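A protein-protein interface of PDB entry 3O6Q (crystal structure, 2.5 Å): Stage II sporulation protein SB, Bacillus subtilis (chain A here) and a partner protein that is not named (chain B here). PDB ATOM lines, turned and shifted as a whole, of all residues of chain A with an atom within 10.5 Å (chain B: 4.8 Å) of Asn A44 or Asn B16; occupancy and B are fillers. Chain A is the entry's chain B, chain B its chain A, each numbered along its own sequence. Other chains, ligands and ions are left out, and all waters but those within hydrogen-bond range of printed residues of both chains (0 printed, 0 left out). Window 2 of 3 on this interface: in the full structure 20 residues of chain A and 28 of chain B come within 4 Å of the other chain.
OD1 of Asn B16 sits close to OD1 of Asn A44 (2.9 Å).
A ring nitrogen (ND1) of His B20 is in hydrogen-bond range of the backbone carbonyl oxygen (O) of Asn B16 (3.2 Å).
OD1 of Asn A44 lies close to O of Ile A40 (3.4 Å).
Phe A41 touches Asn B16 (CD1 to OD1, 3.8 Å).
Phe A41 touches Leu B19 (CE1 to CB, 3.8 Å).
CE1 of His B20 touches CD1 of Phe A41 (3.5 Å).
Ile A48 touches Glu B13 (CG2 to CD, 3.7 Å).
Asn B16 touches Ile A48.
Printed residues of chain B within 4 Å of Phe A41: Asn B16 (3.8 Å), Leu B19 (3.8 Å) and His B20 (3.5 Å).
Of the printed residues of chain B, Ile A48 touches Glu B13 and Asn B16.
Printed residues of chain A within 4 Å of Glu B13: Ile A48.
No residue of chain A comes within 4 Å of Asn B15.
Of chain A, only Phe A41 (3.8 Å), Asn A44 (2.9 Å) and Ile A48 (3.97 Å) come within 4 Å of Asn B16.
His B20 touches just one residue of chain A: Phe A41.
Of the 16 printed residues of chain A, 3 touch a printed residue of chain B.
Printed residues of chain A that touch a printed residue of chain B: Phe A41, Asn A44 and Ile A48.
Of the 9 printed residues of chain B, 4 touch a printed residue of chain A.
Printed residues of chain B that touch a printed residue of chain A: Glu B13, Asn B16, Leu B19 and His B20.
Along chain B the printed residues that touch a printed residue of chain A span positions 13 to 20.
Among the printed residues, no Asp or Glu carboxylate lies within 4 Å of a Lys or Arg side-chain nitrogen of the other chain.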
ATOM      1  N   HIS A  36      -1.424 -27.784 -19.169  1.00  0.00           N
ATOM      2  CA  HIS A  36      -1.990 -28.117 -20.463  1.00  0.00           C
ATOM      3  C   HIS A  36      -3.445 -28.493 -20.313  1.00  0.00           C
ATOM      4  O   HIS A  36      -4.296 -27.969 -21.025  1.00  0.00           O
ATOM      5  CB  HIS A  36      -1.240 -29.299 -21.060  1.00  0.00           C
ATOM      6  CG  HIS A  36      -1.754 -29.726 -22.389  1.00  0.00           C
ATOM      7  ND1 HIS A  36      -2.793 -30.622 -22.530  1.00  0.00           N
ATOM      8  CD2 HIS A  36      -1.374 -29.381 -23.639  1.00  0.00           C
ATOM      9  CE1 HIS A  36      -3.029 -30.807 -23.819  1.00  0.00           C
ATOM     10  NE2 HIS A  36      -2.180 -30.070 -24.513  1.00  0.00           N
ATOM     11  N   THR A  37      -3.738 -29.407 -19.387  1.00  0.00           N
ATOM     12  CA  THR A  37      -5.109 -29.849 -19.240  1.00  0.00           C
ATOM     13  C   THR A  37      -5.927 -28.795 -18.524  1.00  0.00           C
ATOM     14  O   THR A  37      -7.103 -28.659 -18.792  1.00  0.00           O
ATOM     15  CB  THR A  37      -5.287 -31.222 -18.552  1.00  0.00           C
ATOM     16  OG1 THR A  37      -5.427 -31.024 -17.160  1.00  0.00           O
ATOM     17  CG2 THR A  37      -4.164 -32.175 -18.856  1.00  0.00           C
ATOM     18  N   ALA A  38      -5.301 -27.985 -17.681  1.00  0.00           N
ATOM     19  CA  ALA A  38      -6.023 -26.865 -17.060  1.00  0.00           C
ATOM     20  C   ALA A  38      -6.570 -25.907 -18.111  1.00  0.00           C
ATOM     21  O   ALA A  38      -7.676 -25.385 -17.976  1.00  0.00           O
ATOM     22  CB  ALA A  38      -5.102 -26.109 -16.084  1.00  0.00           C
ATOM     23  N   ARG A  39      -5.758 -25.636 -19.128  1.00  0.00           N
ATOM     24  CA  ARG A  39      -6.149 -24.775 -20.239  1.00  0.00           C
ATOM     25  C   ARG A  39      -7.311 -25.345 -21.036  1.00  0.00           C
ATOM     26  O   ARG A  39      -8.217 -24.612 -21.438  1.00  0.00           O
ATOM     27  CB  ARG A  39      -5.006 -24.614 -21.205  1.00  0.00           C
ATOM     28  CG  ARG A  39      -3.922 -23.735 -20.716  1.00  0.00           C
ATOM     29  CD  ARG A  39      -2.768 -23.820 -21.705  1.00  0.00           C
ATOM     30  NE  ARG A  39      -1.489 -23.422 -21.099  1.00  0.00           N
ATOM     31  CZ  ARG A  39      -0.325 -24.052 -21.272  1.00  0.00           C
ATOM     32  NH1 ARG A  39      -0.210 -25.157 -22.025  1.00  0.00           N
ATOM     33  NH2 ARG A  39       0.753 -23.571 -20.667  1.00  0.00           N
ATOM     34  N   ILE A  40      -7.243 -26.651 -21.297  1.00  0.00           N
ATOM     35  CA  ILE A  40      -8.269 -27.329 -22.043  1.00  0.00           C
ATOM     36  C   ILE A  40      -9.556 -27.271 -21.279  1.00  0.00           C
ATOM     37  O   ILE A  40     -10.592 -26.981 -21.855  1.00  0.00           O
ATOM     38  CB  ILE A  40      -7.919 -28.775 -22.289  1.00  0.00           C
ATOM     39  CG1 ILE A  40      -6.849 -28.881 -23.352  1.00  0.00           C
ATOM     40  CG2 ILE A  40      -9.131 -29.547 -22.734  1.00  0.00           C
ATOM     41  CD1 ILE A  40      -6.286 -30.289 -23.446  1.00  0.00           C
ATOM     42  N   PHE A  41      -9.515 -27.536 -19.981  1.00  0.00           N
ATOM     43  CA  PHE A  41     -10.742 -27.424 -19.184  1.00  0.00           C
ATOM     44  C   PHE A  41     -11.300 -26.009 -19.182  1.00  0.00           C
ATOM     45  O   PHE A  41     -12.507 -25.836 -19.377  1.00  0.00           O
ATOM     46  CB  PHE A  41     -10.525 -27.864 -17.746  1.00  0.00           C
ATOM     47  CG  PHE A  41     -10.369 -29.358 -17.576  1.00  0.00           C
ATOM     48  CD1 PHE A  41     -10.922 -30.250 -18.470  1.00  0.00           C
ATOM     49  CD2 PHE A  41      -9.712 -29.863 -16.464  1.00  0.00           C
ATOM     50  CE1 PHE A  41     -10.782 -31.599 -18.273  1.00  0.00           C
ATOM     51  CE2 PHE A  41      -9.578 -31.223 -16.272  1.00  0.00           C
ATOM     52  CZ  PHE A  41     -10.116 -32.085 -17.171  1.00  0.00           C
ATOM     53  N   LYS A  42     -10.439 -25.011 -18.992  1.00  0.00           N
ATOM     54  CA  LYS A  42     -10.901 -23.611 -18.992  1.00  0.00           C
ATOM     55  C   LYS A  42     -11.517 -23.179 -20.319  1.00  0.00           C
ATOM     56  O   LYS A  42     -12.573 -22.551 -20.345  1.00  0.00           O
ATOM     57  CB  LYS A  42      -9.783 -22.627 -18.589  1.00  0.00           C
ATOM     58  CG  LYS A  42      -9.684 -22.371 -17.060  1.00  0.00           C
ATOM     59  CD  LYS A  42     -11.087 -21.989 -16.395  1.00  0.00           C
ATOM     60  CE  LYS A  42     -11.752 -23.161 -15.623  1.00  0.00           C
ATOM     61  NZ  LYS A  42     -13.137 -22.798 -15.152  1.00  0.00           N
ATOM     62  N   GLU A  43     -10.848 -23.512 -21.414  1.00  0.00           N
ATOM     63  CA  GLU A  43     -11.328 -23.140 -22.714  1.00  0.00           C
ATOM     64  C   GLU A  43     -12.642 -23.853 -23.038  1.00  0.00           C
ATOM     65  O   GLU A  43     -13.577 -23.235 -23.557  1.00  0.00           O
ATOM     66  CB  GLU A  43     -10.260 -23.402 -23.768  1.00  0.00           C
ATOM     67  CG  GLU A  43     -10.479 -22.655 -25.082  1.00  0.00           C
ATOM     68  CD  GLU A  43     -10.590 -21.115 -24.982  1.00  0.00           C
ATOM     69  OE1 GLU A  43     -10.067 -20.461 -24.036  1.00  0.00           O
ATOM     70  OE2 GLU A  43     -11.198 -20.566 -25.912  1.00  0.00           O
ATOM     71  N   ASN A  44     -12.739 -25.130 -22.705  1.00  0.00           N
ATOM     72  CA  ASN A  44     -14.002 -25.849 -22.856  1.00  0.00           C
ATOM     73  C   ASN A  44     -15.145 -25.114 -22.198  1.00  0.00           C
ATOM     74  O   ASN A  44     -16.127 -24.809 -22.837  1.00  0.00           O
ATOM     75  CB  ASN A  44     -13.924 -27.246 -22.241  1.00  0.00           C
ATOM     76  CG  ASN A  44     -13.187 -28.232 -23.114  1.00  0.00           C
ATOM     77  OD1 ASN A  44     -12.889 -29.345 -22.684  1.00  0.00           O
ATOM     78  ND2 ASN A  44     -12.884 -27.839 -24.336  1.00  0.00           N
ATOM     79  N   GLU A  45     -14.998 -24.838 -20.914  1.00  0.00           N
ATOM     80  CA  GLU A  45     -16.061 -24.243 -20.116  1.00  0.00           C
ATOM     81  C   GLU A  45     -16.398 -22.834 -20.591  1.00  0.00           C
ATOM     82  O   GLU A  45     -17.551 -22.443 -20.553  1.00  0.00           O
ATOM     83  CB  GLU A  45     -15.684 -24.258 -18.622  1.00  0.00           C
ATOM     84  CG  GLU A  45     -16.671 -23.554 -17.663  1.00  0.00           C
ATOM     85  CD  GLU A  45     -16.242 -22.133 -17.273  1.00  0.00           C
ATOM     86  OE1 GLU A  45     -15.023 -21.847 -17.280  1.00  0.00           O
ATOM     87  OE2 GLU A  45     -17.127 -21.308 -16.943  1.00  0.00           O
ATOM     88  N   ARG A  46     -15.404 -22.087 -21.060  1.00  0.00           N
ATOM     89  CA  ARG A  46     -15.641 -20.742 -21.589  1.00  0.00           C
ATOM     90  C   ARG A  46     -16.364 -20.767 -22.941  1.00  0.00           C
ATOM     91  O   ARG A  46     -17.054 -19.814 -23.290  1.00  0.00           O
ATOM     92  CB  ARG A  46     -14.328 -19.971 -21.700  1.00  0.00           C
ATOM     93  CG  ARG A  46     -13.735 -19.588 -20.339  1.00  0.00           C
ATOM     94  CD  ARG A  46     -12.209 -19.310 -20.413  1.00  0.00           C
ATOM     95  NE  ARG A  46     -11.822 -18.176 -21.268  1.00  0.00           N
ATOM     96  CZ  ARG A  46     -10.573 -17.942 -21.680  1.00  0.00           C
ATOM     97  NH1 ARG A  46     -10.318 -16.888 -22.456  1.00  0.00           N
ATOM     98  NH2 ARG A  46      -9.581 -18.762 -21.340  1.00  0.00           N
ATOM     99  N   LEU A  47     -16.206 -21.850 -23.699  1.00  0.00           N
ATOM    100  CA  LEU A  47     -16.912 -22.022 -24.976  1.00  0.00           C
ATOM    101  C   LEU A  47     -18.308 -22.561 -24.769  1.00  0.00           C
ATOM    102  O   LEU A  47     -19.241 -22.125 -25.421  1.00  0.00           O
ATOM    103  CB  LEU A  47     -16.177 -22.982 -25.900  1.00  0.00           C
ATOM    104  CG  LEU A  47     -15.180 -22.359 -26.846  1.00  0.00           C
ATOM    105  CD1 LEU A  47     -14.577 -23.459 -27.694  1.00  0.00           C
ATOM    106  CD2 LEU A  47     -15.878 -21.347 -27.732  1.00  0.00           C
ATOM    107  N   ILE A  48     -18.442 -23.526 -23.873  1.00  0.00           N
ATOM    108  CA  ILE A  48     -19.739 -24.079 -23.516  1.00  0.00           C
ATOM    109  C   ILE A  48     -20.647 -22.952 -23.004  1.00  0.00           C
ATOM    110  O   ILE A  48     -21.828 -22.887 -23.351  1.00  0.00           O
ATOM    111  CB  ILE A  48     -19.579 -25.191 -22.467  1.00  0.00           C
ATOM    112  CG1 ILE A  48     -18.884 -26.399 -23.114  1.00  0.00           C
ATOM    113  CG2 ILE A  48     -20.926 -25.629 -21.927  1.00  0.00           C
ATOM    114  CD1 ILE A  48     -18.248 -27.353 -22.149  1.00  0.00           C
ATOM    115  N   ASP A  49     -20.067 -22.055 -22.210  1.00  0.00           N
ATOM    116  CA  ASP A  49     -20.727 -20.814 -21.762  1.00  0.00           C
ATOM    117  C   ASP A  49     -21.135 -19.893 -22.907  1.00  0.00           C
ATOM    118  O   ASP A  49     -22.030 -19.066 -22.755  1.00  0.00           O
ATOM    119  CB  ASP A  49     -19.765 -20.000 -20.888  1.00  0.00           C
ATOM    120  CG  ASP A  49     -20.448 -19.310 -19.724  1.00  0.00           C
ATOM    121  OD1 ASP A  49     -21.191 -18.329 -19.971  1.00  0.00           O
ATOM    122  OD2 ASP A  49     -20.212 -19.738 -18.561  1.00  0.00           O
ATOM    123  N   GLU A  50     -20.432 -19.984 -24.024  1.00  0.00           N
ATOM    124  CA  GLU A  50     -20.606 -19.021 -25.087  1.00  0.00           C
ATOM    125  C   GLU A  50     -21.733 -19.338 -26.059  1.00  0.00           C
ATOM    126  O   GLU A  50     -21.967 -18.589 -26.999  1.00  0.00           O
ATOM    127  CB  GLU A  50     -19.258 -18.699 -25.743  1.00  0.00           C
ATOM    128  CG  GLU A  50     -18.529 -17.585 -24.963  1.00  0.00           C
ATOM    129  CD  GLU A  50     -17.191 -17.169 -25.552  1.00  0.00           C
ATOM    130  OE1 GLU A  50     -17.198 -16.522 -26.627  1.00  0.00           O
ATOM    131  OE2 GLU A  50     -16.141 -17.468 -24.915  1.00  0.00           O
ATOM    132  N   TYR A  51     -22.491 -20.398 -25.806  1.00  0.00           N
ATOM    133  CA  TYR A  51     -23.755 -20.570 -26.512  1.00  0.00           C
ATOM    134  C   TYR A  51     -24.915 -20.280 -25.573  1.00  0.00           C
ATOM    135  O   TYR A  51     -25.145 -19.129 -25.206  1.00  0.00           O
ATOM    136  CB  TYR A  51     -23.865 -21.977 -27.072  1.00  0.00           C
ATOM    137  CG  TYR A  51     -22.653 -22.420 -27.860  1.00  0.00           C
ATOM    138  CD1 TYR A  51     -22.559 -22.185 -29.227  1.00  0.00           C
ATOM    139  CD2 TYR A  51     -21.614 -23.080 -27.242  1.00  0.00           C
ATOM    140  CE1 TYR A  51     -21.455 -22.598 -29.947  1.00  0.00           C
ATOM    141  CE2 TYR A  51     -20.513 -23.496 -27.951  1.00  0.00           C
ATOM    142  CZ  TYR A  51     -20.436 -23.251 -29.298  1.00  0.00           C
ATOM    143  OH  TYR A  51     -19.326 -23.665 -29.987  1.00  0.00           O
ATOM    144  N   LEU B  12     -18.965 -31.033 -27.401  1.00  0.00           N
ATOM    145  CA  LEU B  12     -17.971 -30.360 -26.587  1.00  0.00           C
ATOM    146  C   LEU B  12     -18.192 -30.652 -25.100  1.00  0.00           C
ATOM    147  O   LEU B  12     -17.235 -30.932 -24.367  1.00  0.00           O
ATOM    148  CB  LEU B  12     -18.084 -28.865 -26.848  1.00  0.00           C
ATOM    149  CG  LEU B  12     -16.880 -27.953 -26.897  1.00  0.00           C
ATOM    150  CD1 LEU B  12     -15.827 -28.569 -27.794  1.00  0.00           C
ATOM    151  CD2 LEU B  12     -17.339 -26.603 -27.416  1.00  0.00           C
ATOM    152  N   GLU B  13     -19.449 -30.595 -24.668  1.00  0.00           N
ATOM    153  CA  GLU B  13     -19.833 -30.984 -23.317  1.00  0.00           C
ATOM    154  C   GLU B  13     -19.535 -32.466 -23.095  1.00  0.00           C
ATOM    155  O   GLU B  13     -19.117 -32.869 -22.002  1.00  0.00           O
ATOM    156  CB  GLU B  13     -21.319 -30.680 -23.046  1.00  0.00           C
ATOM    157  CG  GLU B  13     -21.555 -29.417 -22.182  1.00  0.00           C
ATOM    158  CD  GLU B  13     -22.866 -28.692 -22.469  1.00  0.00           C
ATOM    159  OE1 GLU B  13     -23.062 -28.269 -23.628  1.00  0.00           O
ATOM    160  OE2 GLU B  13     -23.693 -28.509 -21.542  1.00  0.00           O
ATOM    161  N   GLU B  14     -19.740 -33.283 -24.124  1.00  0.00           N
ATOM    162  CA  GLU B  14     -19.444 -34.722 -23.996  1.00  0.00           C
ATOM    163  C   GLU B  14     -17.945 -34.962 -23.853  1.00  0.00           C
ATOM    164  O   GLU B  14     -17.539 -35.752 -23.029  1.00  0.00           O
ATOM    165  CB  GLU B  14     -19.975 -35.522 -25.184  1.00  0.00           C
ATOM    166  CG  GLU B  14     -20.698 -36.811 -24.800  1.00  0.00           C
ATOM    167  CD  GLU B  14     -21.712 -37.232 -25.847  1.00  0.00           C
ATOM    168  OE1 GLU B  14     -21.642 -36.737 -26.998  1.00  0.00           O
ATOM    169  OE2 GLU B  14     -22.593 -38.053 -25.512  1.00  0.00           O
ATOM    170  N   ASN B  15     -17.126 -34.273 -24.652  1.00  0.00           N
ATOM    171  CA  ASN B  15     -15.647 -34.371 -24.524  1.00  0.00           C
ATOM    172  C   ASN B  15     -15.208 -33.906 -23.149  1.00  0.00           C
ATOM    173  O   ASN B  15     -14.489 -34.601 -22.461  1.00  0.00           O
ATOM    174  CB  ASN B  15     -14.930 -33.543 -25.593  1.00  0.00           C
ATOM    175  CG  ASN B  15     -14.819 -34.280 -26.917  1.00  0.00           C
ATOM    176  OD1 ASN B  15     -15.282 -33.800 -27.954  1.00  0.00           O
ATOM    177  ND2 ASN B  15     -14.246 -35.480 -26.875  1.00  0.00           N
ATOM    178  N   ASN B  16     -15.731 -32.758 -22.733  1.00  0.00           N
ATOM    179  CA  ASN B  16     -15.403 -32.181 -21.456  1.00  0.00           C
ATOM    180  C   ASN B  16     -15.768 -33.094 -20.282  1.00  0.00           C
ATOM    181  O   ASN B  16     -14.957 -33.302 -19.387  1.00  0.00           O
ATOM    182  CB  ASN B  16     -16.104 -30.832 -21.311  1.00  0.00           C
ATOM    183  CG  ASN B  16     -15.492 -29.987 -20.251  1.00  0.00           C
ATOM    184  OD1 ASN B  16     -14.278 -29.836 -20.211  1.00  0.00           O
ATOM    185  ND2 ASN B  16     -16.314 -29.435 -19.371  1.00  0.00           N
ATOM    186  N   GLU B  17     -16.978 -33.635 -20.314  1.00  0.00           N
ATOM    187  CA  GLU B  17     -17.442 -34.587 -19.323  1.00  0.00           C
ATOM    188  C   GLU B  17     -16.544 -35.816 -19.280  1.00  0.00           C
ATOM    189  O   GLU B  17     -16.100 -36.203 -18.206  1.00  0.00           O
ATOM    190  CB  GLU B  17     -18.889 -34.969 -19.595  1.00  0.00           C
ATOM    191  CG  GLU B  17     -19.418 -36.211 -18.850  1.00  0.00           C
ATOM    192  CD  GLU B  17     -20.277 -37.078 -19.784  1.00  0.00           C
ATOM    193  OE1 GLU B  17     -21.513 -36.886 -19.799  1.00  0.00           O
ATOM    194  OE2 GLU B  17     -19.708 -37.903 -20.550  1.00  0.00           O
ATOM    195  N   MET B  18     -16.254 -36.415 -20.431  1.00  0.00           N
ATOM    196  CA  MET B  18     -15.351 -37.576 -20.510  1.00  0.00           C
ATOM    197  C   MET B  18     -13.992 -37.303 -19.849  1.00  0.00           C
ATOM    198  O   MET B  18     -13.463 -38.158 -19.136  1.00  0.00           O
ATOM    199  CB  MET B  18     -15.087 -37.944 -21.973  1.00  0.00           C
ATOM    200  CG  MET B  18     -16.254 -38.582 -22.721  1.00  0.00           C
ATOM    201  SD  MET B  18     -16.385 -40.490 -22.351  1.00  0.00           S
ATOM    202  CE  MET B  18     -14.786 -41.208 -23.206  1.00  0.00           C
ATOM    203  N   LEU B  19     -13.406 -36.141 -20.125  1.00  0.00           N
ATOM    204  CA  LEU B  19     -12.048 -35.862 -19.658  1.00  0.00           C
ATOM    205  C   LEU B  19     -12.019 -35.612 -18.164  1.00  0.00           C
ATOM    206  O   LEU B  19     -11.097 -36.046 -17.482  1.00  0.00           O
ATOM    207  CB  LEU B  19     -11.460 -34.644 -20.361  1.00  0.00           C
ATOM    208  CG  LEU B  19     -10.954 -34.850 -21.806  1.00  0.00           C
ATOM    209  CD1 LEU B  19     -10.817 -33.524 -22.581  1.00  0.00           C
ATOM    210  CD2 LEU B  19      -9.640 -35.689 -21.815  1.00  0.00           C
ATOM    211  N   HIS B  20     -13.038 -34.932 -17.664  1.00  0.00           N
ATOM    212  CA  HIS B  20     -13.178 -34.698 -16.235  1.00  0.00           C
ATOM    213  C   HIS B  20     -13.404 -35.984 -15.497  1.00  0.00           C
ATOM    214  O   HIS B  20     -12.718 -36.285 -14.510  1.00  0.00           O
ATOM    215  CB  HIS B  20     -14.330 -33.748 -15.956  1.00  0.00           C
ATOM    216  CG  HIS B  20     -13.921 -32.323 -15.887  1.00  0.00           C
ATOM    217  ND1 HIS B  20     -14.252 -31.409 -16.859  1.00  0.00           N
ATOM    218  CD2 HIS B  20     -13.214 -31.643 -14.954  1.00  0.00           C
ATOM    219  CE1 HIS B  20     -13.774 -30.220 -16.526  1.00  0.00           C
ATOM    220  NE2 HIS B  20     -13.135 -30.335 -15.377  1.00  0.00           N
